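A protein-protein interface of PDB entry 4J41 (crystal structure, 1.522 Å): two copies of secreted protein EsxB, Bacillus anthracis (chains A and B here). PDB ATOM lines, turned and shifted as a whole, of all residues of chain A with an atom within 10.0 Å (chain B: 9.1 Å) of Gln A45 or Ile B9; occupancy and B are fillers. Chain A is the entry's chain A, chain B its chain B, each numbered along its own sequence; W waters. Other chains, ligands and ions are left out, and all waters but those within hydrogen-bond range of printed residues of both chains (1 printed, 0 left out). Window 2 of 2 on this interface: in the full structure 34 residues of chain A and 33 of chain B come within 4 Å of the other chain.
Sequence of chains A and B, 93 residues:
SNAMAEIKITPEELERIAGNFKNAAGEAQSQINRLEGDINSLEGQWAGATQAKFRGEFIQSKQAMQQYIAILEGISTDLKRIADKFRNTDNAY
Asp A38 touches Ile B17 (CB to CG2, 3.8 Å).
CD2 of Leu A42 touches CD1 of Ile B17, at 3.8 Å.
O of Gln A45 touches CG2 of Ile B9, 3.4 Å away.
Trp A46 touches Leu B14.
Leu B79 touches Trp A46 (CD2 to CH2, 3.8 Å).
Trp A46 touches Ile B82.
CD1 of Ile B82 touches CG2 of Thr A50 (3.6 Å).
Leu B79 touches Phe A54 (CD2 to CE1, 3.6 Å).
Ile B82 touches Phe A54.
No position is printed for both chains.
Hydrophobic or aromatic side chains of chain B that line the printed part of chain A: Ile B9, Leu B14, Ile B17, Leu B79 and Ile B82.
Of the 17 printed residues of chain A, 6 touch a printed residue of chain B.
Printed residues of chain A that touch a printed residue of chain B: Asp A38, Leu A42, Gln A45, Trp A46, Thr A50 and Phe A54.
Among the printed residues, no Asp or Glu carboxylate lies within 4 Å of a Lys or Arg side-chain nitrogen of the other chain.
Water W1 bridges the side-chain carboxylate of Glu B13 and the side-chain hydroxyl of Ser A41.
O of Glu A43 is in hydrogen-bond range of NE2 of Gln A45, at 3.1 Å.
NE1 of Trp A46 lies within hydrogen-bond range of OE1 of Gln A51 (2.8 Å).
The backbone carbonyl oxygen (O) of Asp A38 lies within hydrogen-bond range of the side-chain hydroxyl (OG) of Ser A41, at 2.7 Å.
Gln A45 touches just one residue of chain B: Ile B9 (3.4 Å).
Ile B9 touches just one residue of chain A: Gln A45 (3.4 Å).
No residue of chain B comes within 4 Å of Gly A44.
No residue of chain A comes within 4 Å of Lys B8.
Printed residues of chain A within 4 Å of Leu B14: Trp A46 (3.7 Å).
Of the printed residues of chain B, Trp A46 touches Leu B14 (3.7 Å), Leu B79 (3.8 Å) and Ile B82 (3.8 Å).
Phe B86 touches none of the printed residues of chain A.
The nearest residue of chain B that does not touch Gln A45 is Phe B86 (5.6 Å).
The nearest residue of chain A that does not touch Ile B9 is Trp A46 (4.03 Å).
The nearest printed residue of chain A that does not touch Ile B17 is Ser A41 (4.1 Å).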
ATOM      1  N   GLY A  37      14.861 -14.572   5.506  1.00  0.00           N
ATOM      2  CA  GLY A  37      14.890 -13.339   6.277  1.00  0.00           C
ATOM      3  C   GLY A  37      14.213 -13.511   7.623  1.00  0.00           C
ATOM      4  O   GLY A  37      14.659 -12.938   8.617  1.00  0.00           O
ATOM      5  N   ASP A  38      13.139 -14.302   7.659  1.00  0.00           N
ATOM      6  CA  ASP A  38      12.418 -14.542   8.908  1.00  0.00           C
ATOM      7  C   ASP A  38      13.287 -15.327   9.895  1.00  0.00           C
ATOM      8  O   ASP A  38      13.380 -14.969  11.074  1.00  0.00           O
ATOM      9  CB  ASP A  38      11.110 -15.304   8.665  1.00  0.00           C
ATOM     10  CG  ASP A  38       9.994 -14.426   8.118  1.00  0.00           C
ATOM     11  OD1 ASP A  38      10.083 -13.178   8.209  1.00  0.00           O
ATOM     12  OD2 ASP A  38       9.000 -15.001   7.633  1.00  0.00           O
ATOM     13  N   ILE A  39      13.919 -16.401   9.432  1.00  0.00           N
ATOM     14  CA  ILE A  39      14.807 -17.160  10.316  1.00  0.00           C
ATOM     15  C   ILE A  39      15.991 -16.296  10.761  1.00  0.00           C
ATOM     16  O   ILE A  39      16.392 -16.302  11.941  1.00  0.00           O
ATOM     17  CB  ILE A  39      15.307 -18.459   9.646  1.00  0.00           C
ATOM     18  CG1 ILE A  39      14.127 -19.351   9.251  1.00  0.00           C
ATOM     19  CG2 ILE A  39      16.248 -19.217  10.574  1.00  0.00           C
ATOM     20  CD1 ILE A  39      13.195 -19.679  10.408  1.00  0.00           C
ATOM     21  N   ASN A  40      16.526 -15.516   9.829  1.00  0.00           N
ATOM     22  CA  ASN A  40      17.601 -14.574  10.144  1.00  0.00           C
ATOM     23  C   ASN A  40      17.219 -13.581  11.243  1.00  0.00           C
ATOM     24  O   ASN A  40      18.054 -13.212  12.066  1.00  0.00           O
ATOM     25  CB  ASN A  40      18.040 -13.830   8.868  1.00  0.00           C
ATOM     26  CG  ASN A  40      18.714 -14.744   7.863  1.00  0.00           C
ATOM     27  OD1 ASN A  40      18.856 -15.945   8.102  1.00  0.00           O
ATOM     28  ND2 ASN A  40      19.120 -14.183   6.723  1.00  0.00           N
ATOM     29  N   SER A  41      15.956 -13.165  11.273  1.00  0.00           N
ATOM     30  CA  SER A  41      15.520 -12.150  12.233  1.00  0.00           C
ATOM     31  C   SER A  41      15.522 -12.685  13.658  1.00  0.00           C
ATOM     32  O   SER A  41      15.499 -11.908  14.615  1.00  0.00           O
ATOM     33  CB  SER A  41      14.139 -11.601  11.872  1.00  0.00           C
ATOM     34  OG  SER A  41      13.120 -12.548  12.131  1.00  0.00           O
ATOM     35  N   LEU A  42      15.550 -14.007  13.790  1.00  0.00           N
ATOM     36  CA  LEU A  42      15.582 -14.655  15.104  1.00  0.00           C
ATOM     37  C   LEU A  42      17.002 -14.843  15.627  1.00  0.00           C
ATOM     38  O   LEU A  42      17.197 -15.125  16.815  1.00  0.00           O
ATOM     39  CB  LEU A  42      14.872 -16.011  15.042  1.00  0.00           C
ATOM     40  CG  LEU A  42      13.433 -15.945  14.521  1.00  0.00           C
ATOM     41  CD1 LEU A  42      12.835 -17.331  14.338  1.00  0.00           C
ATOM     42  CD2 LEU A  42      12.579 -15.110  15.457  1.00  0.00           C
ATOM     43  N   GLU A  43      17.991 -14.668  14.758  1.00  0.00           N
ATOM     44  CA  GLU A  43      19.389 -14.910  15.136  1.00  0.00           C
ATOM     45  C   GLU A  43      19.824 -14.067  16.329  1.00  0.00           C
ATOM     46  O   GLU A  43      19.742 -12.833  16.298  1.00  0.00           O
ATOM     47  CB  GLU A  43      20.329 -14.646  13.950  1.00  0.00           C
ATOM     48  CG  GLU A  43      21.785 -15.004  14.239  1.00  0.00           C
ATOM     49  CD  GLU A  43      21.971 -16.485  14.524  1.00  0.00           C
ATOM     50  OE1 GLU A  43      21.795 -17.299  13.600  1.00  0.00           O
ATOM     51  OE2 GLU A  43      22.276 -16.839  15.683  1.00  0.00           O
ATOM     52  N   GLY A  44      20.278 -14.749  17.381  1.00  0.00           N
ATOM     53  CA  GLY A  44      20.789 -14.097  18.572  1.00  0.00           C
ATOM     54  C   GLY A  44      19.711 -13.617  19.522  1.00  0.00           C
ATOM     55  O   GLY A  44      20.021 -13.047  20.568  1.00  0.00           O
ATOM     56  N   GLN A  45      18.447 -13.846  19.171  1.00  0.00           N
ATOM     57  CA  GLN A  45      17.328 -13.370  19.990  1.00  0.00           C
ATOM     58  C   GLN A  45      16.738 -14.483  20.848  1.00  0.00           C
ATOM     59  O   GLN A  45      15.858 -14.240  21.673  1.00  0.00           O
ATOM     60  CB  GLN A  45      16.225 -12.764  19.117  1.00  0.00           C
ATOM     61  CG  GLN A  45      16.722 -11.804  18.051  1.00  0.00           C
ATOM     62  CD  GLN A  45      17.564 -10.691  18.629  1.00  0.00           C
ATOM     63  OE1 GLN A  45      17.194 -10.072  19.628  1.00  0.00           O
ATOM     64  NE2 GLN A  45      18.715 -10.437  18.012  1.00  0.00           N
ATOM     65  N   TRP A  46      17.199 -15.706  20.615  1.00  0.00           N
ATOM     66  CA  TRP A  46      16.856 -16.849  21.461  1.00  0.00           C
ATOM     67  C   TRP A  46      18.027 -17.826  21.538  1.00  0.00           C
ATOM     68  O   TRP A  46      19.082 -17.567  20.965  1.00  0.00           O
ATOM     69  CB  TRP A  46      15.550 -17.532  21.019  1.00  0.00           C
ATOM     70  CG  TRP A  46      15.517 -18.075  19.609  1.00  0.00           C
ATOM     71  CD1 TRP A  46      16.526 -18.062  18.683  1.00  0.00           C
ATOM     72  CD2 TRP A  46      14.398 -18.711  18.972  1.00  0.00           C
ATOM     73  NE1 TRP A  46      16.099 -18.653  17.508  1.00  0.00           N
ATOM     74  CE2 TRP A  46      14.801 -19.059  17.664  1.00  0.00           C
ATOM     75  CE3 TRP A  46      13.098 -19.021  19.382  1.00  0.00           C
ATOM     76  CZ2 TRP A  46      13.945 -19.703  16.768  1.00  0.00           C
ATOM     77  CZ3 TRP A  46      12.254 -19.658  18.491  1.00  0.00           C
ATOM     78  CH2 TRP A  46      12.678 -19.989  17.202  1.00  0.00           C
ATOM     79  N   ALA A  47      17.857 -18.921  22.281  1.00  0.00           N
ATOM     80  CA  ALA A  47      18.957 -19.841  22.550  1.00  0.00           C
ATOM     81  C   ALA A  47      19.596 -20.357  21.262  1.00  0.00           C
ATOM     82  O   ALA A  47      18.897 -20.648  20.281  1.00  0.00           O
ATOM     83  CB  ALA A  47      18.482 -20.998  23.406  1.00  0.00           C
ATOM     84  N   GLY A  48      20.923 -20.452  21.266  1.00  0.00           N
ATOM     85  CA  GLY A  48      21.653 -20.953  20.114  1.00  0.00           C
ATOM     86  C   GLY A  48      21.234 -22.341  19.662  1.00  0.00           C
ATOM     87  O   GLY A  48      21.200 -22.626  18.470  1.00  0.00           O
ATOM     88  N   ALA A  49      20.912 -23.211  20.614  1.00  0.00           N
ATOM     89  CA  ALA A  49      20.454 -24.550  20.273  1.00  0.00           C
ATOM     90  C   ALA A  49      19.115 -24.504  19.544  1.00  0.00           C
ATOM     91  O   ALA A  49      18.865 -25.296  18.639  1.00  0.00           O
ATOM     92  CB  ALA A  49      20.355 -25.409  21.532  1.00  0.00           C
ATOM     93  N   THR A  50      18.257 -23.568  19.942  1.00  0.00           N
ATOM     94  CA  THR A  50      16.966 -23.400  19.282  1.00  0.00           C
ATOM     95  C   THR A  50      17.166 -22.865  17.869  1.00  0.00           C
ATOM     96  O   THR A  50      16.581 -23.383  16.909  1.00  0.00           O
ATOM     97  CB  THR A  50      16.041 -22.472  20.087  1.00  0.00           C
ATOM     98  OG1 THR A  50      15.905 -22.991  21.416  1.00  0.00           O
ATOM     99  CG2 THR A  50      14.663 -22.375  19.434  1.00  0.00           C
ATOM    100  N   GLN A  51      18.004 -21.840  17.737  1.00  0.00           N
ATOM    101  CA  GLN A  51      18.294 -21.288  16.413  1.00  0.00           C
ATOM    102  C   GLN A  51      18.903 -22.346  15.500  1.00  0.00           C
ATOM    103  O   GLN A  51      18.572 -22.413  14.311  1.00  0.00           O
ATOM    104  CB  GLN A  51      19.222 -20.072  16.505  1.00  0.00           C
ATOM    105  CG  GLN A  51      19.582 -19.436  15.147  1.00  0.00           C
ATOM    106  CD  GLN A  51      18.419 -18.710  14.476  1.00  0.00           C
ATOM    107  OE1 GLN A  51      17.294 -18.696  14.977  1.00  0.00           O
ATOM    108  NE2 GLN A  51      18.691 -18.112  13.311  1.00  0.00           N
ATOM    109  N   ALA A  52      19.777 -23.177  16.061  1.00  0.00           N
ATOM    110  CA  ALA A  52      20.457 -24.210  15.283  1.00  0.00           C
ATOM    111  C   ALA A  52      19.466 -25.218  14.715  1.00  0.00           C
ATOM    112  O   ALA A  52      19.601 -25.659  13.577  1.00  0.00           O
ATOM    113  CB  ALA A  52      21.497 -24.916  16.133  1.00  0.00           C
ATOM    114  N   PHE A  54      16.242 -24.655  13.967  1.00  0.00           N
ATOM    115  CA  PHE A  54      15.500 -24.040  12.879  1.00  0.00           C
ATOM    116  C   PHE A  54      16.356 -23.752  11.654  1.00  0.00           C
ATOM    117  O   PHE A  54      15.888 -23.908  10.528  1.00  0.00           O
ATOM    118  CB  PHE A  54      14.745 -22.799  13.353  1.00  0.00           C
ATOM    119  CG  PHE A  54      13.527 -23.129  14.158  1.00  0.00           C
ATOM    120  CD1 PHE A  54      12.346 -23.498  13.526  1.00  0.00           C
ATOM    121  CD2 PHE A  54      13.570 -23.113  15.536  1.00  0.00           C
ATOM    122  CE1 PHE A  54      11.226 -23.823  14.265  1.00  0.00           C
ATOM    123  CE2 PHE A  54      12.455 -23.436  16.278  1.00  0.00           C
ATOM    124  CZ  PHE A  54      11.282 -23.793  15.644  1.00  0.00           C
ATOM    125  N   LYS B   8      11.607  -7.396  18.678  1.00  0.00           N
ATOM    126  CA  LYS B   8      11.737  -8.287  19.827  1.00  0.00           C
ATOM    127  C   LYS B   8      10.972  -9.592  19.619  1.00  0.00           C
ATOM    128  O   LYS B   8       9.860  -9.598  19.083  1.00  0.00           O
ATOM    129  CB  LYS B   8      11.253  -7.585  21.099  1.00  0.00           C
ATOM    130  CG  LYS B   8      11.326  -8.435  22.365  1.00  0.00           C
ATOM    131  CD  LYS B   8      11.257  -7.568  23.615  1.00  0.00           C
ATOM    132  CE  LYS B   8       9.963  -7.775  24.386  1.00  0.00           C
ATOM    133  NZ  LYS B   8       9.911  -9.095  25.071  1.00  0.00           N
ATOM    134  N   ILE B   9      11.564 -10.705  20.038  1.00  0.00           N
ATOM    135  CA  ILE B   9      10.869 -11.980  19.927  1.00  0.00           C
ATOM    136  C   ILE B   9       9.842 -12.190  21.058  1.00  0.00           C
ATOM    137  O   ILE B   9      10.162 -12.212  22.253  1.00  0.00           O
ATOM    138  CB  ILE B   9      11.846 -13.172  19.715  1.00  0.00           C
ATOM    139  CG1 ILE B   9      11.088 -14.395  19.210  1.00  0.00           C
ATOM    140  CG2 ILE B   9      12.667 -13.455  20.960  1.00  0.00           C
ATOM    141  CD1 ILE B   9      11.172 -15.556  20.131  1.00  0.00           C
ATOM    142  N   THR B  10       8.586 -12.274  20.636  1.00  0.00           N
ATOM    143  CA  THR B  10       7.436 -12.442  21.503  1.00  0.00           C
ATOM    144  C   THR B  10       6.667 -13.650  20.985  1.00  0.00           C
ATOM    145  O   THR B  10       6.931 -14.113  19.874  1.00  0.00           O
ATOM    146  CB  THR B  10       6.523 -11.209  21.403  1.00  0.00           C
ATOM    147  OG1 THR B  10       6.119 -11.048  20.042  1.00  0.00           O
ATOM    148  CG2 THR B  10       7.255  -9.957  21.842  1.00  0.00           C
ATOM    149  N   PRO B  11       5.708 -14.172  21.767  1.00  0.00           N
ATOM    150  CA  PRO B  11       4.907 -15.273  21.214  1.00  0.00           C
ATOM    151  C   PRO B  11       4.164 -14.852  19.947  1.00  0.00           C
ATOM    152  O   PRO B  11       4.034 -15.647  19.010  1.00  0.00           O
ATOM    153  CB  PRO B  11       3.921 -15.594  22.345  1.00  0.00           C
ATOM    154  CG  PRO B  11       4.628 -15.141  23.594  1.00  0.00           C
ATOM    155  CD  PRO B  11       5.416 -13.928  23.195  1.00  0.00           C
ATOM    156  N   GLU B  12       3.712 -13.604  19.910  1.00  0.00           N
ATOM    157  CA  GLU B  12       2.999 -13.061  18.759  1.00  0.00           C
ATOM    158  C   GLU B  12       3.884 -12.982  17.529  1.00  0.00           C
ATOM    159  O   GLU B  12       3.423 -13.230  16.411  1.00  0.00           O
ATOM    160  CB  GLU B  12       2.450 -11.671  19.093  1.00  0.00           C
ATOM    161  CG  GLU B  12       1.295 -11.676  20.084  1.00  0.00           C
ATOM    162  CD  GLU B  12       1.729 -11.876  21.529  1.00  0.00           C
ATOM    163  OE1 GLU B  12       2.932 -11.727  21.852  1.00  0.00           O
ATOM    164  OE2 GLU B  12       0.845 -12.181  22.356  1.00  0.00           O
ATOM    165  N   GLU B  13       5.149 -12.626  17.714  1.00  0.00           N
ATOM    166  CA  GLU B  13       6.066 -12.576  16.577  1.00  0.00           C
ATOM    167  C   GLU B  13       6.381 -13.977  16.051  1.00  0.00           C
ATOM    168  O   GLU B  13       6.449 -14.190  14.836  1.00  0.00           O
ATOM    169  CB  GLU B  13       7.348 -11.814  16.936  1.00  0.00           C
ATOM    170  CG  GLU B  13       8.409 -11.798  15.834  1.00  0.00           C
ATOM    171  CD  GLU B  13       8.013 -11.028  14.574  1.00  0.00           C
ATOM    172  OE1 GLU B  13       6.882 -10.495  14.485  1.00  0.00           O
ATOM    173  OE2 GLU B  13       8.851 -10.958  13.646  1.00  0.00           O
ATOM    174  N   LEU B  14       6.561 -14.937  16.953  1.00  0.00           N
ATOM    175  CA  LEU B  14       6.788 -16.319  16.537  1.00  0.00           C
ATOM    176  C   LEU B  14       5.580 -16.863  15.797  1.00  0.00           C
ATOM    177  O   LEU B  14       5.722 -17.604  14.829  1.00  0.00           O
ATOM    178  CB  LEU B  14       7.081 -17.204  17.746  1.00  0.00           C
ATOM    179  CG  LEU B  14       8.427 -16.974  18.419  1.00  0.00           C
ATOM    180  CD1 LEU B  14       8.528 -17.803  19.698  1.00  0.00           C
ATOM    181  CD2 LEU B  14       9.551 -17.320  17.457  1.00  0.00           C
ATOM    182  N   GLU B  15       4.393 -16.499  16.265  1.00  0.00           N
ATOM    183  CA  GLU B  15       3.163 -16.919  15.606  1.00  0.00           C
ATOM    184  C   GLU B  15       3.014 -16.272  14.233  1.00  0.00           C
ATOM    185  O   GLU B  15       2.492 -16.898  13.298  1.00  0.00           O
ATOM    186  CB  GLU B  15       1.952 -16.651  16.509  1.00  0.00           C
ATOM    187  CG  GLU B  15       1.871 -17.658  17.655  1.00  0.00           C
ATOM    188  CD  GLU B  15       0.946 -17.239  18.781  1.00  0.00           C
ATOM    189  OE1 GLU B  15       0.567 -16.050  18.842  1.00  0.00           O
ATOM    190  OE2 GLU B  15       0.606 -18.108  19.614  1.00  0.00           O
ATOM    191  N   ILE B  17       5.529 -15.429  12.254  1.00  0.00           N
ATOM    192  CA  ILE B  17       6.473 -16.123  11.388  1.00  0.00           C
ATOM    193  C   ILE B  17       5.966 -17.524  11.068  1.00  0.00           C
ATOM    194  O   ILE B  17       6.109 -17.999   9.932  1.00  0.00           O
ATOM    195  CB  ILE B  17       7.886 -16.165  12.023  1.00  0.00           C
ATOM    196  CG1 ILE B  17       8.433 -14.737  12.123  1.00  0.00           C
ATOM    197  CG2 ILE B  17       8.837 -17.043  11.205  1.00  0.00           C
ATOM    198  CD1 ILE B  17       9.705 -14.623  12.953  1.00  0.00           C
ATOM    199  N   LEU B  79       7.354 -23.650  15.513  1.00  0.00           N
ATOM    200  CA  LEU B  79       7.355 -22.249  15.934  1.00  0.00           C
ATOM    201  C   LEU B  79       6.162 -21.970  16.832  1.00  0.00           C
ATOM    202  O   LEU B  79       6.292 -21.269  17.835  1.00  0.00           O
ATOM    203  CB  LEU B  79       7.342 -21.303  14.727  1.00  0.00           C
ATOM    204  CG  LEU B  79       8.663 -21.197  13.963  1.00  0.00           C
ATOM    205  CD1 LEU B  79       8.442 -20.410  12.681  1.00  0.00           C
ATOM    206  CD2 LEU B  79       9.736 -20.539  14.795  1.00  0.00           C
ATOM    207  N   ILE B  82       6.868 -23.397  20.281  1.00  0.00           N
ATOM    208  CA  ILE B  82       7.785 -22.560  21.050  1.00  0.00           C
ATOM    209  C   ILE B  82       7.102 -21.270  21.487  1.00  0.00           C
ATOM    210  O   ILE B  82       7.352 -20.776  22.585  1.00  0.00           O
ATOM    211  CB  ILE B  82       9.084 -22.272  20.267  1.00  0.00           C
ATOM    212  CG1 ILE B  82       9.801 -23.586  19.968  1.00  0.00           C
ATOM    213  CG2 ILE B  82      10.005 -21.361  21.048  1.00  0.00           C
ATOM    214  CD1 ILE B  82      11.183 -23.409  19.399  1.00  0.00           C
ATOM    215  N   ALA B  83       6.222 -20.734  20.644  1.00  0.00           N
ATOM    216  CA  ALA B  83       5.469 -19.541  21.017  1.00  0.00           C
ATOM    217  C   ALA B  83       4.635 -19.792  22.265  1.00  0.00           C
ATOM    218  O   ALA B  83       4.572 -18.945  23.153  1.00  0.00           O
ATOM    219  CB  ALA B  83       4.584 -19.095  19.873  1.00  0.00           C
ATOM    220  N   PHE B  86       6.926 -19.830  25.227  1.00  0.00           N
ATOM    221  CA  PHE B  86       7.283 -18.451  25.554  1.00  0.00           C
ATOM    222  C   PHE B  86       6.161 -17.787  26.323  1.00  0.00           C
ATOM    223  O   PHE B  86       6.390 -17.102  27.323  1.00  0.00           O
ATOM    224  CB  PHE B  86       7.539 -17.651  24.274  1.00  0.00           C
ATOM    225  CG  PHE B  86       8.963 -17.662  23.830  1.00  0.00           C
ATOM    226  CD1 PHE B  86       9.613 -18.853  23.581  1.00  0.00           C
ATOM    227  CD2 PHE B  86       9.655 -16.476  23.663  1.00  0.00           C
ATOM    228  CE1 PHE B  86      10.936 -18.868  23.176  1.00  0.00           C
ATOM    229  CE2 PHE B  86      10.976 -16.486  23.262  1.00  0.00           C
ATOM    230  CZ  PHE B  86      11.610 -17.685  23.003  1.00  0.00           C
ATOM    231  N   ARG B  87       4.937 -17.988  25.850  1.00  0.00           N
ATOM    232  CA  ARG B  87       3.780 -17.377  26.492  1.00  0.00           C
ATOM    233  C   ARG B  87       3.632 -17.870  27.936  1.00  0.00           C
ATOM    234  O   ARG B  87       3.121 -17.147  28.799  1.00  0.00           O
ATOM    235  CB  ARG B  87       2.513 -17.633  25.662  1.00  0.00           C
ATOM    236  CG  ARG B  87       1.330 -16.763  26.067  1.00  0.00           C
ATOM    237  CD  ARG B  87       0.177 -16.871  25.074  1.00  0.00           C
ATOM    238  NE  ARG B  87       0.297 -15.920  23.969  1.00  0.00           N
ATOM    239  CZ  ARG B  87       0.459 -16.268  22.696  1.00  0.00           C
ATOM    240  NH1 ARG B  87       0.518 -17.551  22.361  1.00  0.00           N
ATOM    241  NH2 ARG B  87       0.554 -15.333  21.758  1.00  0.00           N
ATOM    242  N   ASP B  90       7.158 -16.208  29.875  1.00  0.00           N
ATOM    243  CA  ASP B  90       7.206 -14.752  29.927  1.00  0.00           C
ATOM    244  C   ASP B  90       6.519 -14.205  31.159  1.00  0.00           C
ATOM    245  O   ASP B  90       5.621 -14.840  31.722  1.00  0.00           O
ATOM    246  CB  ASP B  90       6.492 -14.197  28.684  1.00  0.00           C
ATOM    247  CG  ASP B  90       7.370 -13.283  27.853  1.00  0.00           C
ATOM    248  OD1 ASP B  90       7.932 -12.320  28.415  1.00  0.00           O
ATOM    249  OD2 ASP B  90       7.484 -13.525  26.632  1.00  0.00           O
HETATM  250  O   HOH W   1      11.489 -11.495  14.229  1.00  0.00           O
